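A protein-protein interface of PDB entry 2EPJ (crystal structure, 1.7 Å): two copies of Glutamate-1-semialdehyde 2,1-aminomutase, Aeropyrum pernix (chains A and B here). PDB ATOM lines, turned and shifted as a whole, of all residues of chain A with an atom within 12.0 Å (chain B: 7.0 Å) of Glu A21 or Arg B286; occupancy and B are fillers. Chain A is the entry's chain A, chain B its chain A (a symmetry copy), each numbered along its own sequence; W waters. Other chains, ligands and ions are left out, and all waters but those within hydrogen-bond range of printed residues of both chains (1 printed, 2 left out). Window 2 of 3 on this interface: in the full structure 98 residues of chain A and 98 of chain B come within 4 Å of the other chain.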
ATOM      1  N   SER A  12      19.883  24.168  20.395  1.00  0.00           N
ATOM      2  CA  SER A  12      19.597  22.863  20.988  1.00  0.00           C
ATOM      3  C   SER A  12      20.415  21.799  20.259  1.00  0.00           C
ATOM      4  O   SER A  12      20.895  20.846  20.871  1.00  0.00           O
ATOM      5  CB  SER A  12      18.107  22.524  20.896  1.00  0.00           C
ATOM      6  OG  SER A  12      17.378  23.144  21.942  1.00  0.00           O
ATOM      7  N   ARG A  13      20.574  21.968  18.949  1.00  0.00           N
ATOM      8  CA  ARG A  13      21.351  21.017  18.160  1.00  0.00           C
ATOM      9  C   ARG A  13      22.796  20.990  18.653  1.00  0.00           C
ATOM     10  O   ARG A  13      23.386  19.920  18.808  1.00  0.00           O
ATOM     11  CB  ARG A  13      21.326  21.394  16.676  1.00  0.00           C
ATOM     12  CG  ARG A  13      22.127  20.441  15.792  1.00  0.00           C
ATOM     13  CD  ARG A  13      22.194  20.930  14.350  1.00  0.00           C
ATOM     14  NE  ARG A  13      22.796  22.258  14.246  1.00  0.00           N
ATOM     15  CZ  ARG A  13      24.040  22.552  14.616  1.00  0.00           C
ATOM     16  NH1 ARG A  13      24.829  21.610  15.117  1.00  0.00           N
ATOM     17  NH2 ARG A  13      24.494  23.793  14.490  1.00  0.00           N
ATOM     18  N   MET A  14      23.362  22.168  18.902  1.00  0.00           N
ATOM     19  CA  MET A  14      24.735  22.262  19.382  1.00  0.00           C
ATOM     20  C   MET A  14      24.893  21.572  20.735  1.00  0.00           C
ATOM     21  O   MET A  14      25.852  20.833  20.952  1.00  0.00           O
ATOM     22  CB  MET A  14      25.168  23.725  19.492  1.00  0.00           C
ATOM     23  CG  MET A  14      25.204  24.459  18.159  1.00  0.00           C
ATOM     24  SD  MET A  14      25.885  26.123  18.306  1.00  0.00           S
ATOM     25  CE  MET A  14      24.442  27.034  18.812  1.00  0.00           C
ATOM     26  N   LEU A  15      23.956  21.821  21.645  1.00  0.00           N
ATOM     27  CA  LEU A  15      24.000  21.201  22.962  1.00  0.00           C
ATOM     28  C   LEU A  15      23.843  19.691  22.831  1.00  0.00           C
ATOM     29  O   LEU A  15      24.462  18.924  23.573  1.00  0.00           O
ATOM     30  CB  LEU A  15      22.901  21.782  23.857  1.00  0.00           C
ATOM     31  CG  LEU A  15      23.193  23.210  24.326  1.00  0.00           C
ATOM     32  CD1 LEU A  15      21.946  23.844  24.928  1.00  0.00           C
ATOM     33  CD2 LEU A  15      24.330  23.179  25.341  1.00  0.00           C
ATOM     34  N   PHE A  16      23.019  19.269  21.876  1.00  0.00           N
ATOM     35  CA  PHE A  16      22.787  17.852  21.623  1.00  0.00           C
ATOM     36  C   PHE A  16      24.111  17.179  21.262  1.00  0.00           C
ATOM     37  O   PHE A  16      24.410  16.076  21.721  1.00  0.00           O
ATOM     38  CB  PHE A  16      21.792  17.686  20.471  1.00  0.00           C
ATOM     39  CG  PHE A  16      21.494  16.254  20.126  1.00  0.00           C
ATOM     40  CD1 PHE A  16      20.724  15.464  20.975  1.00  0.00           C
ATOM     41  CD2 PHE A  16      21.987  15.692  18.952  1.00  0.00           C
ATOM     42  CE1 PHE A  16      20.449  14.135  20.659  1.00  0.00           C
ATOM     43  CE2 PHE A  16      21.719  14.365  18.628  1.00  0.00           C
ATOM     44  CZ  PHE A  16      20.947  13.585  19.485  1.00  0.00           C
ATOM     45  N   GLU A  17      24.905  17.854  20.439  1.00  0.00           N
ATOM     46  CA  GLU A  17      26.196  17.320  20.024  1.00  0.00           C
ATOM     47  C   GLU A  17      27.168  17.226  21.196  1.00  0.00           C
ATOM     48  O   GLU A  17      27.888  16.237  21.333  1.00  0.00           O
ATOM     49  CB  GLU A  17      26.807  18.195  18.924  1.00  0.00           C
ATOM     50  CG  GLU A  17      26.062  18.152  17.599  1.00  0.00           C
ATOM     51  CD  GLU A  17      25.913  16.739  17.062  1.00  0.00           C
ATOM     52  OE1 GLU A  17      26.922  16.004  17.030  1.00  0.00           O
ATOM     53  OE2 GLU A  17      24.786  16.368  16.666  1.00  0.00           O
ATOM     54  N   ARG A  18      27.181  18.254  22.040  1.00  0.00           N
ATOM     55  CA  ARG A  18      28.075  18.294  23.193  1.00  0.00           C
ATOM     56  C   ARG A  18      27.791  17.227  24.243  1.00  0.00           C
ATOM     57  O   ARG A  18      28.715  16.676  24.839  1.00  0.00           O
ATOM     58  CB  ARG A  18      28.021  19.675  23.857  1.00  0.00           C
ATOM     59  CG  ARG A  18      28.750  20.756  23.084  1.00  0.00           C
ATOM     60  CD  ARG A  18      28.433  22.144  23.613  1.00  0.00           C
ATOM     61  NE  ARG A  18      28.895  22.363  24.981  1.00  0.00           N
ATOM     62  CZ  ARG A  18      28.772  23.522  25.621  1.00  0.00           C
ATOM     63  NH1 ARG A  18      28.204  24.556  25.014  1.00  0.00           N
ATOM     64  NH2 ARG A  18      29.214  23.654  26.863  1.00  0.00           N
ATOM     65  N   THR A  19      26.517  16.930  24.469  1.00  0.00           N
ATOM     66  CA  THR A  19      26.152  15.946  25.485  1.00  0.00           C
ATOM     67  C   THR A  19      26.285  14.492  25.045  1.00  0.00           C
ATOM     68  O   THR A  19      26.312  13.588  25.880  1.00  0.00           O
ATOM     69  CB  THR A  19      24.716  16.191  25.999  1.00  0.00           C
ATOM     70  OG1 THR A  19      23.792  16.141  24.905  1.00  0.00           O
ATOM     71  CG2 THR A  19      24.622  17.557  26.671  1.00  0.00           C
ATOM     72  N   LYS A  20      26.382  14.264  23.739  1.00  0.00           N
ATOM     73  CA  LYS A  20      26.514  12.908  23.217  1.00  0.00           C
ATOM     74  C   LYS A  20      27.649  12.136  23.884  1.00  0.00           C
ATOM     75  O   LYS A  20      27.513  10.949  24.177  1.00  0.00           O
ATOM     76  CB  LYS A  20      26.748  12.947  21.705  1.00  0.00           C
ATOM     77  CG  LYS A  20      25.498  13.225  20.888  1.00  0.00           C
ATOM     78  CD  LYS A  20      25.813  13.522  19.420  1.00  0.00           C
ATOM     79  CE  LYS A  20      26.637  12.423  18.758  1.00  0.00           C
ATOM     80  NZ  LYS A  20      28.056  12.417  19.220  1.00  0.00           N
ATOM     81  N   GLU A  21      28.763  12.815  24.127  1.00  0.00           N
ATOM     82  CA  GLU A  21      29.923  12.179  24.743  1.00  0.00           C
ATOM     83  C   GLU A  21      30.064  12.462  26.236  1.00  0.00           C
ATOM     84  O   GLU A  21      31.000  11.978  26.874  1.00  0.00           O
ATOM     85  CB  GLU A  21      31.201  12.619  24.021  1.00  0.00           C
ATOM     86  CG  GLU A  21      31.290  12.156  22.573  1.00  0.00           C
ATOM     87  CD  GLU A  21      32.501  12.716  21.855  1.00  0.00           C
ATOM     88  OE1 GLU A  21      32.587  13.954  21.713  1.00  0.00           O
ATOM     89  OE2 GLU A  21      33.368  11.920  21.430  1.00  0.00           O
ATOM     90  N   LEU A  22      29.139  13.239  26.792  1.00  0.00           N
ATOM     91  CA  LEU A  22      29.191  13.583  28.210  1.00  0.00           C
ATOM     92  C   LEU A  22      28.300  12.711  29.084  1.00  0.00           C
ATOM     93  O   LEU A  22      28.680  12.346  30.200  1.00  0.00           O
ATOM     94  CB  LEU A  22      28.777  15.041  28.427  1.00  0.00           C
ATOM     95  CG  LEU A  22      29.654  16.183  27.915  1.00  0.00           C
ATOM     96  CD1 LEU A  22      28.954  17.498  28.221  1.00  0.00           C
ATOM     97  CD2 LEU A  22      31.029  16.138  28.576  1.00  0.00           C
ATOM     98  N   PHE A  23      27.112  12.397  28.577  1.00  0.00           N
ATOM     99  CA  PHE A  23      26.136  11.600  29.317  1.00  0.00           C
ATOM    100  C   PHE A  23      25.735  10.333  28.574  1.00  0.00           C
ATOM    101  O   PHE A  23      25.647  10.326  27.342  1.00  0.00           O
ATOM    102  CB  PHE A  23      24.848  12.404  29.553  1.00  0.00           C
ATOM    103  CG  PHE A  23      25.063  13.790  30.097  1.00  0.00           C
ATOM    104  CD1 PHE A  23      25.897  14.015  31.186  1.00  0.00           C
ATOM    105  CD2 PHE A  23      24.374  14.871  29.545  1.00  0.00           C
ATOM    106  CE1 PHE A  23      26.045  15.293  31.720  1.00  0.00           C
ATOM    107  CE2 PHE A  23      24.514  16.157  30.073  1.00  0.00           C
ATOM    108  CZ  PHE A  23      25.351  16.369  31.163  1.00  0.00           C
ATOM    109  N   PRO A  24      25.479   9.239  29.310  1.00  0.00           N
ATOM    110  CA  PRO A  24      25.075   8.009  28.625  1.00  0.00           C
ATOM    111  C   PRO A  24      23.742   8.296  27.930  1.00  0.00           C
ATOM    112  O   PRO A  24      22.800   8.777  28.561  1.00  0.00           O
ATOM    113  CB  PRO A  24      24.923   7.008  29.771  1.00  0.00           C
ATOM    114  CG  PRO A  24      25.928   7.496  30.782  1.00  0.00           C
ATOM    115  CD  PRO A  24      25.711   8.994  30.745  1.00  0.00           C
ATOM    116  N   GLY A  25      23.664   8.012  26.633  1.00  0.00           N
ATOM    117  CA  GLY A  25      22.433   8.270  25.910  1.00  0.00           C
ATOM    118  C   GLY A  25      22.189   9.757  25.718  1.00  0.00           C
ATOM    119  O   GLY A  25      21.124  10.164  25.251  1.00  0.00           O
ATOM    120  N   GLY A  26      23.180  10.567  26.091  1.00  0.00           N
ATOM    121  CA  GLY A  26      23.081  12.010  25.946  1.00  0.00           C
ATOM    122  C   GLY A  26      22.185  12.749  26.927  1.00  0.00           C
ATOM    123  O   GLY A  26      21.994  13.957  26.792  1.00  0.00           O
ATOM    124  N   VAL A  27      21.652  12.046  27.926  1.00  0.00           N
ATOM    125  CA  VAL A  27      20.755  12.677  28.901  1.00  0.00           C
ATOM    126  C   VAL A  27      21.000  12.189  30.326  1.00  0.00           C
ATOM    127  O   VAL A  27      21.675  11.181  30.533  1.00  0.00           O
ATOM    128  CB  VAL A  27      19.269  12.392  28.559  1.00  0.00           C
ATOM    129  CG1 VAL A  27      18.909  13.002  27.209  1.00  0.00           C
ATOM    130  CG2 VAL A  27      19.021  10.892  28.539  1.00  0.00           C
ATOM    131  N   ASN A  28      20.447  12.907  31.306  1.00  0.00           N
ATOM    132  CA  ASN A  28      20.604  12.519  32.703  1.00  0.00           C
ATOM    133  C   ASN A  28      19.431  11.705  33.250  1.00  0.00           C
ATOM    134  O   ASN A  28      19.424  11.308  34.415  1.00  0.00           O
ATOM    135  CB  ASN A  28      20.891  13.748  33.567  1.00  0.00           C
ATOM    136  CG  ASN A  28      22.364  14.106  33.569  1.00  0.00           C
ATOM    137  OD1 ASN A  28      23.188  13.374  34.124  1.00  0.00           O
ATOM    138  ND2 ASN A  28      22.712  15.218  32.930  1.00  0.00           N
ATOM    139  N   ALA A  33      15.609  11.649  26.510  1.00  0.00           N
ATOM    140  CA  ALA A  33      16.195  11.365  25.202  1.00  0.00           C
ATOM    141  C   ALA A  33      15.189  11.079  24.089  1.00  0.00           C
ATOM    142  O   ALA A  33      15.530  11.160  22.908  1.00  0.00           O
ATOM    143  CB  ALA A  33      17.163  10.190  25.317  1.00  0.00           C
ATOM    144  N   TYR A  41      16.614  21.947  24.370  1.00  0.00           N
ATOM    145  CA  TYR A  41      17.191  22.344  25.644  1.00  0.00           C
ATOM    146  C   TYR A  41      16.411  23.548  26.140  1.00  0.00           C
ATOM    147  O   TYR A  41      16.001  24.402  25.354  1.00  0.00           O
ATOM    148  CB  TYR A  41      18.682  22.651  25.489  1.00  0.00           C
ATOM    149  CG  TYR A  41      19.510  21.387  25.426  1.00  0.00           C
ATOM    150  CD1 TYR A  41      19.327  20.468  24.394  1.00  0.00           C
ATOM    151  CD2 TYR A  41      20.416  21.070  26.439  1.00  0.00           C
ATOM    152  CE1 TYR A  41      20.018  19.258  24.375  1.00  0.00           C
ATOM    153  CE2 TYR A  41      21.115  19.859  26.428  1.00  0.00           C
ATOM    154  CZ  TYR A  41      20.904  18.960  25.394  1.00  0.00           C
ATOM    155  OH  TYR A  41      21.556  17.749  25.385  1.00  0.00           O
ATOM    156  N   LEU B 106      34.369  16.417  34.623  1.00  0.00           N
ATOM    157  CA  LEU B 106      35.087  15.377  33.894  1.00  0.00           C
ATOM    158  C   LEU B 106      36.512  15.786  33.524  1.00  0.00           C
ATOM    159  O   LEU B 106      37.410  14.947  33.477  1.00  0.00           O
ATOM    160  CB  LEU B 106      34.305  14.975  32.637  1.00  0.00           C
ATOM    161  CG  LEU B 106      33.012  14.192  32.900  1.00  0.00           C
ATOM    162  CD1 LEU B 106      32.228  14.050  31.610  1.00  0.00           C
ATOM    163  CD2 LEU B 106      33.342  12.815  33.477  1.00  0.00           C
ATOM    164  N   LYS B 110      37.873  12.554  35.159  1.00  0.00           N
ATOM    165  CA  LYS B 110      37.813  11.465  34.190  1.00  0.00           C
ATOM    166  C   LYS B 110      37.719  12.025  32.775  1.00  0.00           C
ATOM    167  O   LYS B 110      36.671  11.967  32.133  1.00  0.00           O
ATOM    168  CB  LYS B 110      36.608  10.572  34.494  1.00  0.00           C
ATOM    169  CG  LYS B 110      36.526   9.309  33.653  1.00  0.00           C
ATOM    170  CD  LYS B 110      37.681   8.358  33.924  1.00  0.00           C
ATOM    171  CE  LYS B 110      37.643   7.814  35.342  1.00  0.00           C
ATOM    172  NZ  LYS B 110      38.682   6.766  35.556  1.00  0.00           N
ATOM    173  N   GLY B 112      37.542  12.591  29.037  1.00  0.00           N
ATOM    174  CA  GLY B 112      37.073  11.733  27.964  1.00  0.00           C
ATOM    175  C   GLY B 112      36.021  10.731  28.403  1.00  0.00           C
ATOM    176  O   GLY B 112      35.535   9.943  27.594  1.00  0.00           O
ATOM    177  N   GLY B 113      35.663  10.759  29.682  1.00  0.00           N
ATOM    178  CA  GLY B 113      34.664   9.828  30.179  1.00  0.00           C
ATOM    179  C   GLY B 113      33.260  10.406  30.156  1.00  0.00           C
ATOM    180  O   GLY B 113      32.989  11.374  29.443  1.00  0.00           O
ATOM    181  N   MET B 114      32.366   9.800  30.932  1.00  0.00           N
ATOM    182  CA  MET B 114      30.981  10.253  31.020  1.00  0.00           C
ATOM    183  C   MET B 114      30.570  10.388  32.478  1.00  0.00           C
ATOM    184  O   MET B 114      31.224   9.849  33.371  1.00  0.00           O
ATOM    185  CB  MET B 114      30.038   9.262  30.339  1.00  0.00           C
ATOM    186  CG  MET B 114      30.271   9.078  28.861  1.00  0.00           C
ATOM    187  SD  MET B 114      29.083   7.906  28.184  1.00  0.00           S
ATOM    188  CE  MET B 114      28.600   8.767  26.698  1.00  0.00           C
ATOM    189  N   ILE B 115      29.467  11.088  32.708  1.00  0.00           N
ATOM    190  CA  ILE B 115      28.975  11.295  34.059  1.00  0.00           C
ATOM    191  C   ILE B 115      27.450  11.233  34.080  1.00  0.00           C
ATOM    192  O   ILE B 115      26.794  11.483  33.067  1.00  0.00           O
ATOM    193  CB  ILE B 115      29.460  12.671  34.599  1.00  0.00           C
ATOM    194  CG1 ILE B 115      29.157  12.799  36.094  1.00  0.00           C
ATOM    195  CG2 ILE B 115      28.801  13.807  33.821  1.00  0.00           C
ATOM    196  CD1 ILE B 115      29.847  13.992  36.748  1.00  0.00           C
ATOM    197  N   GLY B 284      32.915   7.844  34.949  1.00  0.00           N
ATOM    198  CA  GLY B 284      33.746   6.720  34.565  1.00  0.00           C
ATOM    199  C   GLY B 284      34.032   6.743  33.080  1.00  0.00           C
ATOM    200  O   GLY B 284      33.636   7.676  32.380  1.00  0.00           O
ATOM    201  N   SER B 285      34.721   5.716  32.593  1.00  0.00           N
ATOM    202  CA  SER B 285      35.051   5.634  31.177  1.00  0.00           C
ATOM    203  C   SER B 285      33.784   5.501  30.347  1.00  0.00           C
ATOM    204  O   SER B 285      32.732   5.108  30.855  1.00  0.00           O
ATOM    205  CB  SER B 285      35.945   4.424  30.912  1.00  0.00           C
ATOM    206  OG  SER B 285      35.252   3.227  31.214  1.00  0.00           O
ATOM    207  N   ARG B 286      33.888   5.833  29.065  1.00  0.00           N
ATOM    208  CA  ARG B 286      32.745   5.717  28.173  1.00  0.00           C
ATOM    209  C   ARG B 286      32.284   4.261  28.126  1.00  0.00           C
ATOM    210  O   ARG B 286      31.085   3.979  28.100  1.00  0.00           O
ATOM    211  CB  ARG B 286      33.120   6.182  26.763  1.00  0.00           C
ATOM    212  CG  ARG B 286      31.974   6.097  25.769  1.00  0.00           C
ATOM    213  CD  ARG B 286      32.413   6.538  24.379  1.00  0.00           C
ATOM    214  NE  ARG B 286      32.947   7.894  24.384  1.00  0.00           N
ATOM    215  CZ  ARG B 286      33.366   8.534  23.297  1.00  0.00           C
ATOM    216  NH1 ARG B 286      33.312   7.939  22.113  1.00  0.00           N
ATOM    217  NH2 ARG B 286      33.843   9.768  23.393  1.00  0.00           N
ATOM    218  N   GLU B 287      33.241   3.338  28.130  1.00  0.00           N
ATOM    219  CA  GLU B 287      32.928   1.916  28.071  1.00  0.00           C
ATOM    220  C   GLU B 287      32.059   1.437  29.225  1.00  0.00           C
ATOM    221  O   GLU B 287      31.137   0.652  29.023  1.00  0.00           O
ATOM    222  CB  GLU B 287      34.214   1.082  28.019  1.00  0.00           C
ATOM    223  CG  GLU B 287      34.985   1.223  26.712  1.00  0.00           C
ATOM    224  CD  GLU B 287      36.005   2.348  26.736  1.00  0.00           C
ATOM    225  OE1 GLU B 287      35.794   3.343  27.462  1.00  0.00           O
ATOM    226  OE2 GLU B 287      37.019   2.239  26.012  1.00  0.00           O
ATOM    227  N   VAL B 288      32.349   1.902  30.434  1.00  0.00           N
ATOM    228  CA  VAL B 288      31.564   1.487  31.587  1.00  0.00           C
ATOM    229  C   VAL B 288      30.265   2.281  31.694  1.00  0.00           C
ATOM    230  O   VAL B 288      29.188   1.705  31.841  1.00  0.00           O
ATOM    231  CB  VAL B 288      32.361   1.652  32.900  1.00  0.00           C
ATOM    232  CG1 VAL B 288      31.469   1.341  34.088  1.00  0.00           C
ATOM    233  CG2 VAL B 288      33.572   0.717  32.897  1.00  0.00           C
ATOM    234  N   MET B 289      30.372   3.601  31.600  1.00  0.00           N
ATOM    235  CA  MET B 289      29.213   4.480  31.715  1.00  0.00           C
ATOM    236  C   MET B 289      28.143   4.284  30.641  1.00  0.00           C
ATOM    237  O   MET B 289      26.971   4.572  30.875  1.00  0.00           O
ATOM    238  CB  MET B 289      29.666   5.946  31.717  1.00  0.00           C
ATOM    239  CG  MET B 289      30.470   6.367  32.951  1.00  0.00           C
ATOM    240  SD  MET B 289      29.567   6.192  34.519  1.00  0.00           S
ATOM    241  CE  MET B 289      28.347   7.508  34.346  1.00  0.00           C
ATOM    242  N   SER B 290      28.538   3.799  29.468  1.00  0.00           N
ATOM    243  CA  SER B 290      27.581   3.592  28.381  1.00  0.00           C
ATOM    244  C   SER B 290      26.538   2.515  28.673  1.00  0.00           C
ATOM    245  O   SER B 290      25.590   2.339  27.906  1.00  0.00           O
ATOM    246  CB  SER B 290      28.317   3.256  27.081  1.00  0.00           C
ATOM    247  OG  SER B 290      28.989   2.015  27.186  1.00  0.00           O
ATOM    248  N   LEU B 291      26.710   1.785  29.771  1.00  0.00           N
ATOM    249  CA  LEU B 291      25.746   0.751  30.135  1.00  0.00           C
ATOM    250  C   LEU B 291      24.495   1.355  30.774  1.00  0.00           C
ATOM    251  O   LEU B 291      23.467   0.696  30.887  1.00  0.00           O
ATOM    252  CB  LEU B 291      26.371  -0.260  31.101  1.00  0.00           C
ATOM    253  CG  LEU B 291      27.129  -1.447  30.494  1.00  0.00           C
ATOM    254  CD1 LEU B 291      28.259  -0.959  29.615  1.00  0.00           C
ATOM    255  CD2 LEU B 291      27.666  -2.324  31.621  1.00  0.00           C
HETATM  256  O   HOH W   1      33.895  13.342  27.760  1.00  0.00           O
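Water W1 lies within hydrogen-bond range of the backbone carbonyl oxygen (O) of Gly B113 (2.7 Å) and the backbone carbonyl oxygen (O) of Glu A21 (3.3 Å).
Of the 14 printed residues of chain B, 6 touch a printed residue of chain A. Among the printed residues, 11 pairs touch across the chains.
Of chain B, only Gly B113 (3.3 Å), Met B114 (3.6 Å) and Arg B286 (3.0 Å) come within 4 Å of Glu A21. Of chain A, only Glu A21 comes within 4 Å of Arg B286. No residue of chain A comes within 4 Å of Gly B112. Printed residues of chain A within 4 Å of Gly B113: Glu A21. No residue of chain A comes within 4 Å of Gly B284. Glu B287 touches none of the printed residues of chain A. Of the printed residues of chain A, Ile B115 touches Leu A22 (2.9 Å), Phe A23 (3.3 Å) and Pro A24 (3.6 Å). Printed residues of chain A within 4 Å of Met B114: Lys A20, Glu A21, Leu A22 and Phe A23. Printed residues of chain B within 4 Å of Leu A22: Leu B106, Met B114 and Ile B115. The nearest residue of chain B that does not touch Glu A21 is Gly B112 (5.0 Å). The nearest residue of chain A that does not touch Arg B286 is Lys A20 (6.2 Å). The nearest printed residue of chain B that does not touch Pro A24 is Met B114 (4.004 Å).
N of Met B114 lies within hydrogen-bond range of O of Gly B284, 2.9 Å away. The backbone NH of Gly B284 lies close to the side-chain sulfur of Met B289 (3.8 Å). The side-chain hydroxyl (OG) of Ser B290 sits at hydrogen-bond distance from the backbone carbonyl oxygen (O) of Arg B286 (3.0 Å).
No position is printed for both chains.
The guanidinium group (NH2) of Arg B286 is in salt-bridge range of the side-chain carboxylate (OE2) of Glu A21. The backbone carbonyl oxygen of Leu A22 sits at hydrogen-bond distance from the backbone NH of Ile B115 (2.9 Å). O of Glu A21 lies close to O of Gly B113 (3.3 Å).
Met B114 touches Lys A20. CG of Met B114 touches O of Glu A21 (3.6 Å). CD2 of Leu A22 touches CD1 of Leu B106, 3.9 Å away. Leu A22 touches Met B114 (O to CA, 3.2 Å). Phe A23 touches Met B114 (O to CE, 3.4 Å). CD1 of Phe A23 touches O of Ile B115, 3.3 Å away. Pro A24 touches Ile B115. Pro A24 touches Met B289 (CG to O, 3.1 Å).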
